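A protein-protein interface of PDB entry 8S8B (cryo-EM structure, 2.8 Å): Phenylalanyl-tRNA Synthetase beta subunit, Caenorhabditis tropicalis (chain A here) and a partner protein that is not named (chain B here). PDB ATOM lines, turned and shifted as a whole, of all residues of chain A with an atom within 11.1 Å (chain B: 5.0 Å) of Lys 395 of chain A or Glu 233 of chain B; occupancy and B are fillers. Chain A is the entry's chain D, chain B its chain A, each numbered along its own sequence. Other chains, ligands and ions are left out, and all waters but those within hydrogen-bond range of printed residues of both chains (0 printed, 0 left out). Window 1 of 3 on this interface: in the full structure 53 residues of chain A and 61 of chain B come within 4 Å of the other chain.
The side-chain carboxylate (OE2) of Glu 403 of chain A is in salt-bridge range of the side-chain amino group (NZ) of Lys 229 of chain B (3.9 Å). The side-chain carboxylate of Glu 233 of chain B lies within salt-bridge range of the side-chain amino group of Lys 395 of chain A, at 3.6 Å.
Among the printed residues, pairs that only touch across the chains: Lys 395 of chain A with Gln 236 of chain B (3.6 Å) and Asn 399 of chain A with Glu 233 of chain B (3.9 Å).
Of chain B, only Glu 233 and Gln 236 come within 4 Å of Lys 395 of chain A. Of the printed residues of chain B, Asn 399 of chain A touches Glu 233 (3.9 Å). Printed residues of chain B within 4 Å of Glu 403 of chain A: Lys 229. Printed residues of chain A within 4 Å of Lys 229 of chain B: Glu 403. No residue of chain A comes within 4 Å of Ser 232 of chain B. Of chain A, only Lys 395 and Asn 399 come within 4 Å of Glu 233 of chain B. Cys 492 of chain B touches none of the printed residues of chain A. The nearest printed residue of chain B that does not touch Lys 395 of chain A is Leu 494 of chain B (5.1 Å). The nearest printed residue of chain B that does not touch Asn 399 of chain A is Cys 492 of chain B (4.4 Å).
Of the 24 printed residues of chain A, 3 touch a printed residue of chain B.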
ATOM      1  N   ALA A 388      -9.671 -35.645  -4.978  1.00  0.00           N
ATOM      2  CA  ALA A 388     -10.527 -34.469  -4.916  1.00  0.00           C
ATOM      3  C   ALA A 388     -11.392 -34.408  -6.165  1.00  0.00           C
ATOM      4  O   ALA A 388     -10.874 -34.429  -7.285  1.00  0.00           O
ATOM      5  CB  ALA A 388      -9.693 -33.195  -4.785  1.00  0.00           C
ATOM      6  N   VAL A 389     -12.705 -34.324  -5.972  1.00  0.00           N
ATOM      7  CA  VAL A 389     -13.667 -34.249  -7.064  1.00  0.00           C
ATOM      8  C   VAL A 389     -14.272 -32.853  -7.077  1.00  0.00           C
ATOM      9  O   VAL A 389     -14.725 -32.354  -6.042  1.00  0.00           O
ATOM     10  CB  VAL A 389     -14.757 -35.326  -6.935  1.00  0.00           C
ATOM     11  CG1 VAL A 389     -14.216 -36.672  -7.367  1.00  0.00           C
ATOM     12  CG2 VAL A 389     -15.257 -35.404  -5.508  1.00  0.00           C
ATOM     13  N   ALA A 390     -14.267 -32.221  -8.244  1.00  0.00           N
ATOM     14  CA  ALA A 390     -14.813 -30.882  -8.385  1.00  0.00           C
ATOM     15  C   ALA A 390     -16.314 -30.940  -8.644  1.00  0.00           C
ATOM     16  O   ALA A 390     -16.878 -31.983  -8.980  1.00  0.00           O
ATOM     17  CB  ALA A 390     -14.110 -30.133  -9.514  1.00  0.00           C
ATOM     18  N   PHE A 391     -16.964 -29.799  -8.474  1.00  0.00           N
ATOM     19  CA  PHE A 391     -18.371 -29.679  -8.831  1.00  0.00           C
ATOM     20  C   PHE A 391     -18.485 -29.408 -10.326  1.00  0.00           C
ATOM     21  O   PHE A 391     -17.914 -28.430 -10.815  1.00  0.00           O
ATOM     22  CB  PHE A 391     -19.032 -28.565  -8.027  1.00  0.00           C
ATOM     23  CG  PHE A 391     -20.518 -28.711  -7.896  1.00  0.00           C
ATOM     24  CD1 PHE A 391     -21.072 -29.898  -7.455  1.00  0.00           C
ATOM     25  CD2 PHE A 391     -21.358 -27.657  -8.196  1.00  0.00           C
ATOM     26  CE1 PHE A 391     -22.438 -30.034  -7.332  1.00  0.00           C
ATOM     27  CE2 PHE A 391     -22.725 -27.787  -8.075  1.00  0.00           C
ATOM     28  CZ  PHE A 391     -23.265 -28.977  -7.643  1.00  0.00           C
ATOM     29  N   PRO A 392     -19.200 -30.251 -11.079  1.00  0.00           N
ATOM     30  CA  PRO A 392     -19.088 -30.197 -12.549  1.00  0.00           C
ATOM     31  C   PRO A 392     -19.439 -28.853 -13.161  1.00  0.00           C
ATOM     32  O   PRO A 392     -18.765 -28.410 -14.104  1.00  0.00           O
ATOM     33  CB  PRO A 392     -20.063 -31.293 -13.003  1.00  0.00           C
ATOM     34  CG  PRO A 392     -20.180 -32.208 -11.833  1.00  0.00           C
ATOM     35  CD  PRO A 392     -20.086 -31.334 -10.628  1.00  0.00           C
ATOM     36  N   ILE A 393     -20.471 -28.180 -12.650  1.00  0.00           N
ATOM     37  CA  ILE A 393     -20.883 -26.920 -13.256  1.00  0.00           C
ATOM     38  C   ILE A 393     -19.813 -25.855 -13.047  1.00  0.00           C
ATOM     39  O   ILE A 393     -19.563 -25.033 -13.933  1.00  0.00           O
ATOM     40  CB  ILE A 393     -22.258 -26.482 -12.715  1.00  0.00           C
ATOM     41  CG1 ILE A 393     -22.735 -25.218 -13.428  1.00  0.00           C
ATOM     42  CG2 ILE A 393     -22.216 -26.265 -11.222  1.00  0.00           C
ATOM     43  CD1 ILE A 393     -22.956 -25.403 -14.909  1.00  0.00           C
ATOM     44  N   ASN A 394     -19.149 -25.865 -11.890  1.00  0.00           N
ATOM     45  CA  ASN A 394     -18.072 -24.909 -11.650  1.00  0.00           C
ATOM     46  C   ASN A 394     -16.907 -25.131 -12.606  1.00  0.00           C
ATOM     47  O   ASN A 394     -16.343 -24.168 -13.139  1.00  0.00           O
ATOM     48  CB  ASN A 394     -17.599 -25.002 -10.201  1.00  0.00           C
ATOM     49  CG  ASN A 394     -18.657 -24.569  -9.213  1.00  0.00           C
ATOM     50  OD1 ASN A 394     -18.931 -25.261  -8.236  1.00  0.00           O
ATOM     51  ND2 ASN A 394     -19.261 -23.414  -9.464  1.00  0.00           N
ATOM     52  N   LYS A 395     -16.532 -26.391 -12.830  1.00  0.00           N
ATOM     53  CA  LYS A 395     -15.442 -26.694 -13.751  1.00  0.00           C
ATOM     54  C   LYS A 395     -15.783 -26.258 -15.170  1.00  0.00           C
ATOM     55  O   LYS A 395     -14.961 -25.626 -15.855  1.00  0.00           O
ATOM     56  CB  LYS A 395     -15.137 -28.189 -13.699  1.00  0.00           C
ATOM     57  CG  LYS A 395     -13.974 -28.639 -14.554  1.00  0.00           C
ATOM     58  CD  LYS A 395     -13.746 -30.133 -14.385  1.00  0.00           C
ATOM     59  CE  LYS A 395     -12.576 -30.613 -15.221  1.00  0.00           C
ATOM     60  NZ  LYS A 395     -11.309 -29.936 -14.836  1.00  0.00           N
ATOM     61  N   LEU A 396     -16.999 -26.574 -15.624  1.00  0.00           N
ATOM     62  CA  LEU A 396     -17.420 -26.145 -16.953  1.00  0.00           C
ATOM     63  C   LEU A 396     -17.431 -24.626 -17.061  1.00  0.00           C
ATOM     64  O   LEU A 396     -16.997 -24.067 -18.073  1.00  0.00           O
ATOM     65  CB  LEU A 396     -18.798 -26.715 -17.280  1.00  0.00           C
ATOM     66  CG  LEU A 396     -19.473 -26.161 -18.536  1.00  0.00           C
ATOM     67  CD1 LEU A 396     -18.655 -26.473 -19.776  1.00  0.00           C
ATOM     68  CD2 LEU A 396     -20.883 -26.704 -18.672  1.00  0.00           C
ATOM     69  N   CYS A 397     -17.917 -23.943 -16.022  1.00  0.00           N
ATOM     70  CA  CYS A 397     -17.970 -22.487 -16.050  1.00  0.00           C
ATOM     71  C   CYS A 397     -16.577 -21.880 -16.107  1.00  0.00           C
ATOM     72  O   CYS A 397     -16.358 -20.902 -16.822  1.00  0.00           O
ATOM     73  CB  CYS A 397     -18.734 -21.969 -14.834  1.00  0.00           C
ATOM     74  SG  CYS A 397     -20.519 -22.217 -14.926  1.00  0.00           S
ATOM     75  N   ASP A 398     -15.624 -22.439 -15.362  1.00  0.00           N
ATOM     76  CA  ASP A 398     -14.261 -21.915 -15.395  1.00  0.00           C
ATOM     77  C   ASP A 398     -13.642 -22.088 -16.778  1.00  0.00           C
ATOM     78  O   ASP A 398     -13.061 -21.145 -17.343  1.00  0.00           O
ATOM     79  CB  ASP A 398     -13.415 -22.615 -14.333  1.00  0.00           C
ATOM     80  CG  ASP A 398     -12.046 -21.992 -14.171  1.00  0.00           C
ATOM     81  OD1 ASP A 398     -11.791 -20.933 -14.783  1.00  0.00           O
ATOM     82  OD2 ASP A 398     -11.221 -22.562 -13.428  1.00  0.00           O
ATOM     83  N   ASN A 399     -13.769 -23.291 -17.347  1.00  0.00           N
ATOM     84  CA  ASN A 399     -13.206 -23.524 -18.672  1.00  0.00           C
ATOM     85  C   ASN A 399     -13.860 -22.629 -19.716  1.00  0.00           C
ATOM     86  O   ASN A 399     -13.184 -22.119 -20.615  1.00  0.00           O
ATOM     87  CB  ASN A 399     -13.346 -24.995 -19.057  1.00  0.00           C
ATOM     88  CG  ASN A 399     -12.343 -25.876 -18.349  1.00  0.00           C
ATOM     89  OD1 ASN A 399     -11.291 -25.412 -17.916  1.00  0.00           O
ATOM     90  ND2 ASN A 399     -12.659 -27.159 -18.235  1.00  0.00           N
ATOM     91  N   LEU A 400     -15.174 -22.419 -19.611  1.00  0.00           N
ATOM     92  CA  LEU A 400     -15.859 -21.554 -20.563  1.00  0.00           C
ATOM     93  C   LEU A 400     -15.463 -20.096 -20.372  1.00  0.00           C
ATOM     94  O   LEU A 400     -15.349 -19.346 -21.346  1.00  0.00           O
ATOM     95  CB  LEU A 400     -17.370 -21.725 -20.422  1.00  0.00           C
ATOM     96  CG  LEU A 400     -18.248 -20.920 -21.377  1.00  0.00           C
ATOM     97  CD1 LEU A 400     -17.945 -21.294 -22.813  1.00  0.00           C
ATOM     98  CD2 LEU A 400     -19.711 -21.151 -21.058  1.00  0.00           C
ATOM     99  N   ARG A 401     -15.249 -19.679 -19.125  1.00  0.00           N
ATOM    100  CA  ARG A 401     -14.897 -18.293 -18.846  1.00  0.00           C
ATOM    101  C   ARG A 401     -13.520 -17.953 -19.390  1.00  0.00           C
ATOM    102  O   ARG A 401     -13.290 -16.820 -19.833  1.00  0.00           O
ATOM    103  CB  ARG A 401     -14.963 -18.047 -17.340  1.00  0.00           C
ATOM    104  CG  ARG A 401     -14.882 -16.598 -16.927  1.00  0.00           C
ATOM    105  CD  ARG A 401     -15.337 -16.436 -15.488  1.00  0.00           C
ATOM    106  NE  ARG A 401     -14.712 -17.417 -14.610  1.00  0.00           N
ATOM    107  CZ  ARG A 401     -13.585 -17.214 -13.941  1.00  0.00           C
ATOM    108  NH1 ARG A 401     -12.933 -16.066 -14.019  1.00  0.00           N
ATOM    109  NH2 ARG A 401     -13.102 -18.186 -13.175  1.00  0.00           N
ATOM    110  N   ILE A 402     -12.597 -18.916 -19.375  1.00  0.00           N
ATOM    111  CA  ILE A 402     -11.297 -18.675 -20.000  1.00  0.00           C
ATOM    112  C   ILE A 402     -11.468 -18.341 -21.480  1.00  0.00           C
ATOM    113  O   ILE A 402     -10.870 -17.386 -21.992  1.00  0.00           O
ATOM    114  CB  ILE A 402     -10.366 -19.883 -19.795  1.00  0.00           C
ATOM    115  CG1 ILE A 402      -9.951 -19.990 -18.330  1.00  0.00           C
ATOM    116  CG2 ILE A 402      -9.145 -19.763 -20.681  1.00  0.00           C
ATOM    117  CD1 ILE A 402      -8.973 -21.107 -18.055  1.00  0.00           C
ATOM    118  N   GLU A 403     -12.304 -19.106 -22.184  1.00  0.00           N
ATOM    119  CA  GLU A 403     -12.533 -18.842 -23.602  1.00  0.00           C
ATOM    120  C   GLU A 403     -13.284 -17.536 -23.823  1.00  0.00           C
ATOM    121  O   GLU A 403     -13.036 -16.839 -24.813  1.00  0.00           O
ATOM    122  CB  GLU A 403     -13.297 -20.001 -24.233  1.00  0.00           C
ATOM    123  CG  GLU A 403     -12.732 -21.370 -23.900  1.00  0.00           C
ATOM    124  CD  GLU A 403     -11.374 -21.617 -24.524  1.00  0.00           C
ATOM    125  OE1 GLU A 403     -11.040 -20.943 -25.520  1.00  0.00           O
ATOM    126  OE2 GLU A 403     -10.639 -22.491 -24.019  1.00  0.00           O
ATOM    127  N   ILE A 404     -14.211 -17.195 -22.924  1.00  0.00           N
ATOM    128  CA  ILE A 404     -14.922 -15.924 -23.041  1.00  0.00           C
ATOM    129  C   ILE A 404     -13.944 -14.765 -22.933  1.00  0.00           C
ATOM    130  O   ILE A 404     -14.022 -13.793 -23.695  1.00  0.00           O
ATOM    131  CB  ILE A 404     -16.032 -15.821 -21.979  1.00  0.00           C
ATOM    132  CG1 ILE A 404     -17.065 -16.926 -22.166  1.00  0.00           C
ATOM    133  CG2 ILE A 404     -16.713 -14.473 -22.063  1.00  0.00           C
ATOM    134  CD1 ILE A 404     -18.130 -16.939 -21.105  1.00  0.00           C
ATOM    135  N   LEU A 477     -21.498 -14.611 -15.779  1.00  0.00           N
ATOM    136  CA  LEU A 477     -22.198 -15.887 -15.637  1.00  0.00           C
ATOM    137  C   LEU A 477     -22.332 -16.175 -14.145  1.00  0.00           C
ATOM    138  O   LEU A 477     -21.342 -16.426 -13.455  1.00  0.00           O
ATOM    139  CB  LEU A 477     -21.486 -17.014 -16.384  1.00  0.00           C
ATOM    140  CG  LEU A 477     -20.027 -17.387 -16.139  1.00  0.00           C
ATOM    141  CD1 LEU A 477     -19.938 -18.596 -15.232  1.00  0.00           C
ATOM    142  CD2 LEU A 477     -19.340 -17.666 -17.459  1.00  0.00           C
ATOM    143  N   ARG A 495     -28.019 -21.331 -12.999  1.00  0.00           N
ATOM    144  CA  ARG A 495     -26.814 -20.695 -13.513  1.00  0.00           C
ATOM    145  C   ARG A 495     -27.054 -20.198 -14.930  1.00  0.00           C
ATOM    146  O   ARG A 495     -27.424 -20.974 -15.813  1.00  0.00           O
ATOM    147  CB  ARG A 495     -25.648 -21.681 -13.490  1.00  0.00           C
ATOM    148  CG  ARG A 495     -24.340 -21.120 -14.007  1.00  0.00           C
ATOM    149  CD  ARG A 495     -23.716 -20.174 -13.007  1.00  0.00           C
ATOM    150  NE  ARG A 495     -23.493 -20.820 -11.722  1.00  0.00           N
ATOM    151  CZ  ARG A 495     -22.361 -21.410 -11.367  1.00  0.00           C
ATOM    152  NH1 ARG A 495     -21.319 -21.447 -12.180  1.00  0.00           N
ATOM    153  NH2 ARG A 495     -22.271 -21.976 -10.168  1.00  0.00           N
ATOM    154  N   MET A 521     -17.517 -23.543 -28.791  1.00  0.00           N
ATOM    155  CA  MET A 521     -16.652 -23.969 -27.696  1.00  0.00           C
ATOM    156  C   MET A 521     -17.289 -25.057 -26.844  1.00  0.00           C
ATOM    157  O   MET A 521     -16.571 -25.771 -26.137  1.00  0.00           O
ATOM    158  CB  MET A 521     -16.275 -22.772 -26.824  1.00  0.00           C
ATOM    159  CG  MET A 521     -15.563 -21.660 -27.576  1.00  0.00           C
ATOM    160  SD  MET A 521     -14.170 -22.251 -28.554  1.00  0.00           S
ATOM    161  CE  MET A 521     -13.128 -22.942 -27.276  1.00  0.00           C
ATOM    162  N   LEU A 522     -18.610 -25.199 -26.892  1.00  0.00           N
ATOM    163  CA  LEU A 522     -19.307 -26.262 -26.183  1.00  0.00           C
ATOM    164  C   LEU A 522     -19.521 -27.502 -27.040  1.00  0.00           C
ATOM    165  O   LEU A 522     -20.167 -28.450 -26.580  1.00  0.00           O
ATOM    166  CB  LEU A 522     -20.654 -25.751 -25.664  1.00  0.00           C
ATOM    167  CG  LEU A 522     -20.584 -24.750 -24.512  1.00  0.00           C
ATOM    168  CD1 LEU A 522     -21.945 -24.143 -24.248  1.00  0.00           C
ATOM    169  CD2 LEU A 522     -20.055 -25.426 -23.263  1.00  0.00           C
ATOM    170  N   VAL A 586     -27.050 -22.403 -18.922  1.00  0.00           N
ATOM    171  CA  VAL A 586     -25.919 -23.257 -19.260  1.00  0.00           C
ATOM    172  C   VAL A 586     -25.952 -24.591 -18.533  1.00  0.00           C
ATOM    173  O   VAL A 586     -24.963 -25.328 -18.578  1.00  0.00           O
ATOM    174  CB  VAL A 586     -24.577 -22.543 -19.006  1.00  0.00           C
ATOM    175  CG1 VAL A 586     -24.458 -21.309 -19.879  1.00  0.00           C
ATOM    176  CG2 VAL A 586     -24.444 -22.178 -17.544  1.00  0.00           C
ATOM    177  N   PHE A 589     -26.227 -27.926 -20.990  1.00  0.00           N
ATOM    178  CA  PHE A 589     -24.968 -28.368 -21.578  1.00  0.00           C
ATOM    179  C   PHE A 589     -24.133 -29.214 -20.628  1.00  0.00           C
ATOM    180  O   PHE A 589     -23.149 -29.816 -21.070  1.00  0.00           O
ATOM    181  CB  PHE A 589     -24.150 -27.164 -22.037  1.00  0.00           C
ATOM    182  CG  PHE A 589     -24.812 -26.361 -23.108  1.00  0.00           C
ATOM    183  CD1 PHE A 589     -24.706 -26.736 -24.433  1.00  0.00           C
ATOM    184  CD2 PHE A 589     -25.536 -25.229 -22.793  1.00  0.00           C
ATOM    185  CE1 PHE A 589     -25.313 -25.997 -25.425  1.00  0.00           C
ATOM    186  CE2 PHE A 589     -26.145 -24.485 -23.780  1.00  0.00           C
ATOM    187  CZ  PHE A 589     -26.033 -24.870 -25.097  1.00  0.00           C
ATOM    188  N   LEU A 590     -24.487 -29.269 -19.351  1.00  0.00           N
ATOM    189  CA  LEU A 590     -23.740 -30.062 -18.386  1.00  0.00           C
ATOM    190  C   LEU A 590     -23.864 -31.545 -18.708  1.00  0.00           C
ATOM    191  O   LEU A 590     -22.975 -32.339 -18.409  1.00  0.00           O
ATOM    192  CB  LEU A 590     -24.233 -29.782 -16.968  1.00  0.00           C
ATOM    193  CG  LEU A 590     -23.487 -30.485 -15.836  1.00  0.00           C
ATOM    194  CD1 LEU A 590     -22.006 -30.178 -15.921  1.00  0.00           C
ATOM    195  CD2 LEU A 590     -24.047 -30.062 -14.491  1.00  0.00           C
ATOM    196  OXT LEU A 590     -24.858 -31.982 -19.286  1.00  0.00           O
ATOM    197  N   LYS B 229      -3.664 -27.911 -23.904  1.00  0.00           N
ATOM    198  CA  LYS B 229      -4.871 -28.068 -23.098  1.00  0.00           C
ATOM    199  C   LYS B 229      -4.921 -29.444 -22.448  1.00  0.00           C
ATOM    200  O   LYS B 229      -5.246 -29.571 -21.259  1.00  0.00           O
ATOM    201  CB  LYS B 229      -6.114 -27.848 -23.957  1.00  0.00           C
ATOM    202  CG  LYS B 229      -6.256 -26.453 -24.523  1.00  0.00           C
ATOM    203  CD  LYS B 229      -7.542 -26.334 -25.322  1.00  0.00           C
ATOM    204  CE  LYS B 229      -7.722 -24.939 -25.885  1.00  0.00           C
ATOM    205  NZ  LYS B 229      -8.957 -24.831 -26.704  1.00  0.00           N
ATOM    206  N   VAL B 230      -4.606 -30.489 -23.215  1.00  0.00           N
ATOM    207  CA  VAL B 230      -4.596 -31.834 -22.651  1.00  0.00           C
ATOM    208  C   VAL B 230      -3.537 -31.945 -21.560  1.00  0.00           C
ATOM    209  O   VAL B 230      -3.755 -32.592 -20.528  1.00  0.00           O
ATOM    210  CB  VAL B 230      -4.388 -32.874 -23.764  1.00  0.00           C
ATOM    211  CG1 VAL B 230      -4.347 -34.267 -23.185  1.00  0.00           C
ATOM    212  CG2 VAL B 230      -5.500 -32.769 -24.789  1.00  0.00           C
ATOM    213  N   ARG B 231      -2.381 -31.311 -21.764  1.00  0.00           N
ATOM    214  CA  ARG B 231      -1.337 -31.335 -20.746  1.00  0.00           C
ATOM    215  C   ARG B 231      -1.796 -30.649 -19.467  1.00  0.00           C
ATOM    216  O   ARG B 231      -1.526 -31.134 -18.362  1.00  0.00           O
ATOM    217  CB  ARG B 231      -0.068 -30.673 -21.282  1.00  0.00           C
ATOM    218  CG  ARG B 231       1.161 -30.925 -20.433  1.00  0.00           C
ATOM    219  CD  ARG B 231       2.404 -30.363 -21.090  1.00  0.00           C
ATOM    220  NE  ARG B 231       2.444 -28.909 -21.027  1.00  0.00           N
ATOM    221  CZ  ARG B 231       3.086 -28.222 -20.092  1.00  0.00           C
ATOM    222  NH1 ARG B 231       3.759 -28.829 -19.129  1.00  0.00           N
ATOM    223  NH2 ARG B 231       3.050 -26.893 -20.125  1.00  0.00           N
ATOM    224  N   SER B 232      -2.487 -29.516 -19.597  1.00  0.00           N
ATOM    225  CA  SER B 232      -3.008 -28.825 -18.421  1.00  0.00           C
ATOM    226  C   SER B 232      -4.027 -29.684 -17.687  1.00  0.00           C
ATOM    227  O   SER B 232      -4.035 -29.734 -16.450  1.00  0.00           O
ATOM    228  CB  SER B 232      -3.628 -27.489 -18.828  1.00  0.00           C
ATOM    229  OG  SER B 232      -2.675 -26.655 -19.462  1.00  0.00           O
ATOM    230  N   GLU B 233      -4.897 -30.366 -18.432  1.00  0.00           N
ATOM    231  CA  GLU B 233      -5.872 -31.250 -17.798  1.00  0.00           C
ATOM    232  C   GLU B 233      -5.184 -32.383 -17.047  1.00  0.00           C
ATOM    233  O   GLU B 233      -5.572 -32.721 -15.921  1.00  0.00           O
ATOM    234  CB  GLU B 233      -6.832 -31.806 -18.848  1.00  0.00           C
ATOM    235  CG  GLU B 233      -8.291 -31.486 -18.586  1.00  0.00           C
ATOM    236  CD  GLU B 233      -8.587 -30.002 -18.658  1.00  0.00           C
ATOM    237  OE1 GLU B 233      -7.852 -29.279 -19.362  1.00  0.00           O
ATOM    238  OE2 GLU B 233      -9.556 -29.557 -18.009  1.00  0.00           O
ATOM    239  N   PHE B 234      -4.156 -32.980 -17.654  1.00  0.00           N
ATOM    240  CA  PHE B 234      -3.414 -34.041 -16.980  1.00  0.00           C
ATOM    241  C   PHE B 234      -2.729 -33.522 -15.722  1.00  0.00           C
ATOM    242  O   PHE B 234      -2.704 -34.207 -14.692  1.00  0.00           O
ATOM    243  CB  PHE B 234      -2.387 -34.651 -17.934  1.00  0.00           C
ATOM    244  CG  PHE B 234      -2.921 -35.786 -18.760  1.00  0.00           C
ATOM    245  CD1 PHE B 234      -3.694 -35.546 -19.880  1.00  0.00           C
ATOM    246  CD2 PHE B 234      -2.635 -37.095 -18.422  1.00  0.00           C
ATOM    247  CE1 PHE B 234      -4.178 -36.588 -20.639  1.00  0.00           C
ATOM    248  CE2 PHE B 234      -3.117 -38.139 -19.181  1.00  0.00           C
ATOM    249  CZ  PHE B 234      -3.888 -37.884 -20.291  1.00  0.00           C
ATOM    250  N   ARG B 235      -2.157 -32.318 -15.792  1.00  0.00           N
ATOM    251  CA  ARG B 235      -1.527 -31.729 -14.616  1.00  0.00           C
ATOM    252  C   ARG B 235      -2.538 -31.521 -13.497  1.00  0.00           C
ATOM    253  O   ARG B 235      -2.246 -31.796 -12.328  1.00  0.00           O
ATOM    254  CB  ARG B 235      -0.862 -30.404 -14.985  1.00  0.00           C
ATOM    255  CG  ARG B 235       0.542 -30.542 -15.539  1.00  0.00           C
ATOM    256  CD  ARG B 235       1.010 -29.244 -16.172  1.00  0.00           C
ATOM    257  NE  ARG B 235       0.638 -28.080 -15.377  1.00  0.00           N
ATOM    258  CZ  ARG B 235       1.380 -27.568 -14.405  1.00  0.00           C
ATOM    259  NH1 ARG B 235       2.546 -28.095 -14.074  1.00  0.00           N
ATOM    260  NH2 ARG B 235       0.939 -26.499 -13.748  1.00  0.00           N
ATOM    261  N   GLN B 236      -3.731 -31.030 -13.837  1.00  0.00           N
ATOM    262  CA  GLN B 236      -4.758 -30.836 -12.819  1.00  0.00           C
ATOM    263  C   GLN B 236      -5.183 -32.160 -12.201  1.00  0.00           C
ATOM    264  O   GLN B 236      -5.391 -32.242 -10.985  1.00  0.00           O
ATOM    265  CB  GLN B 236      -5.960 -30.109 -13.414  1.00  0.00           C
ATOM    266  CG  GLN B 236      -5.699 -28.647 -13.719  1.00  0.00           C
ATOM    267  CD  GLN B 236      -6.928 -27.936 -14.239  1.00  0.00           C
ATOM    268  OE1 GLN B 236      -7.998 -28.529 -14.361  1.00  0.00           O
ATOM    269  NE2 GLN B 236      -6.780 -26.655 -14.548  1.00  0.00           N
ATOM    270  N   ILE B 237      -5.319 -33.207 -13.017  1.00  0.00           N
ATOM    271  CA  ILE B 237      -5.678 -34.517 -12.477  1.00  0.00           C
ATOM    272  C   ILE B 237      -4.603 -35.016 -11.519  1.00  0.00           C
ATOM    273  O   ILE B 237      -4.902 -35.499 -10.417  1.00  0.00           O
ATOM    274  CB  ILE B 237      -5.921 -35.519 -13.620  1.00  0.00           C
ATOM    275  CG1 ILE B 237      -7.133 -35.102 -14.451  1.00  0.00           C
ATOM    276  CG2 ILE B 237      -6.116 -36.916 -13.069  1.00  0.00           C
ATOM    277  CD1 ILE B 237      -7.428 -36.034 -15.601  1.00  0.00           C
ATOM    278  N   CYS B 492     -11.548 -28.703 -23.494  1.00  0.00           N
ATOM    279  CA  CYS B 492     -11.182 -30.084 -23.188  1.00  0.00           C
ATOM    280  C   CYS B 492     -12.117 -30.620 -22.113  1.00  0.00           C
ATOM    281  O   CYS B 492     -11.846 -30.526 -20.917  1.00  0.00           O
ATOM    282  CB  CYS B 492      -9.726 -30.170 -22.754  1.00  0.00           C
ATOM    283  SG  CYS B 492      -9.157 -31.848 -22.415  1.00  0.00           S
ATOM    284  N   LEU B 494     -12.685 -33.749 -21.182  1.00  0.00           N
ATOM    285  CA  LEU B 494     -12.192 -35.117 -21.301  1.00  0.00           C
ATOM    286  C   LEU B 494     -13.047 -36.112 -20.527  1.00  0.00           C
ATOM    287  O   LEU B 494     -13.014 -37.310 -20.830  1.00  0.00           O
ATOM    288  CB  LEU B 494     -10.735 -35.192 -20.838  1.00  0.00           C
ATOM    289  CG  LEU B 494     -10.376 -35.235 -19.349  1.00  0.00           C
ATOM    290  CD1 LEU B 494      -8.867 -35.187 -19.200  1.00  0.00           C
ATOM    291  CD2 LEU B 494     -11.018 -34.113 -18.544  1.00  0.00           C
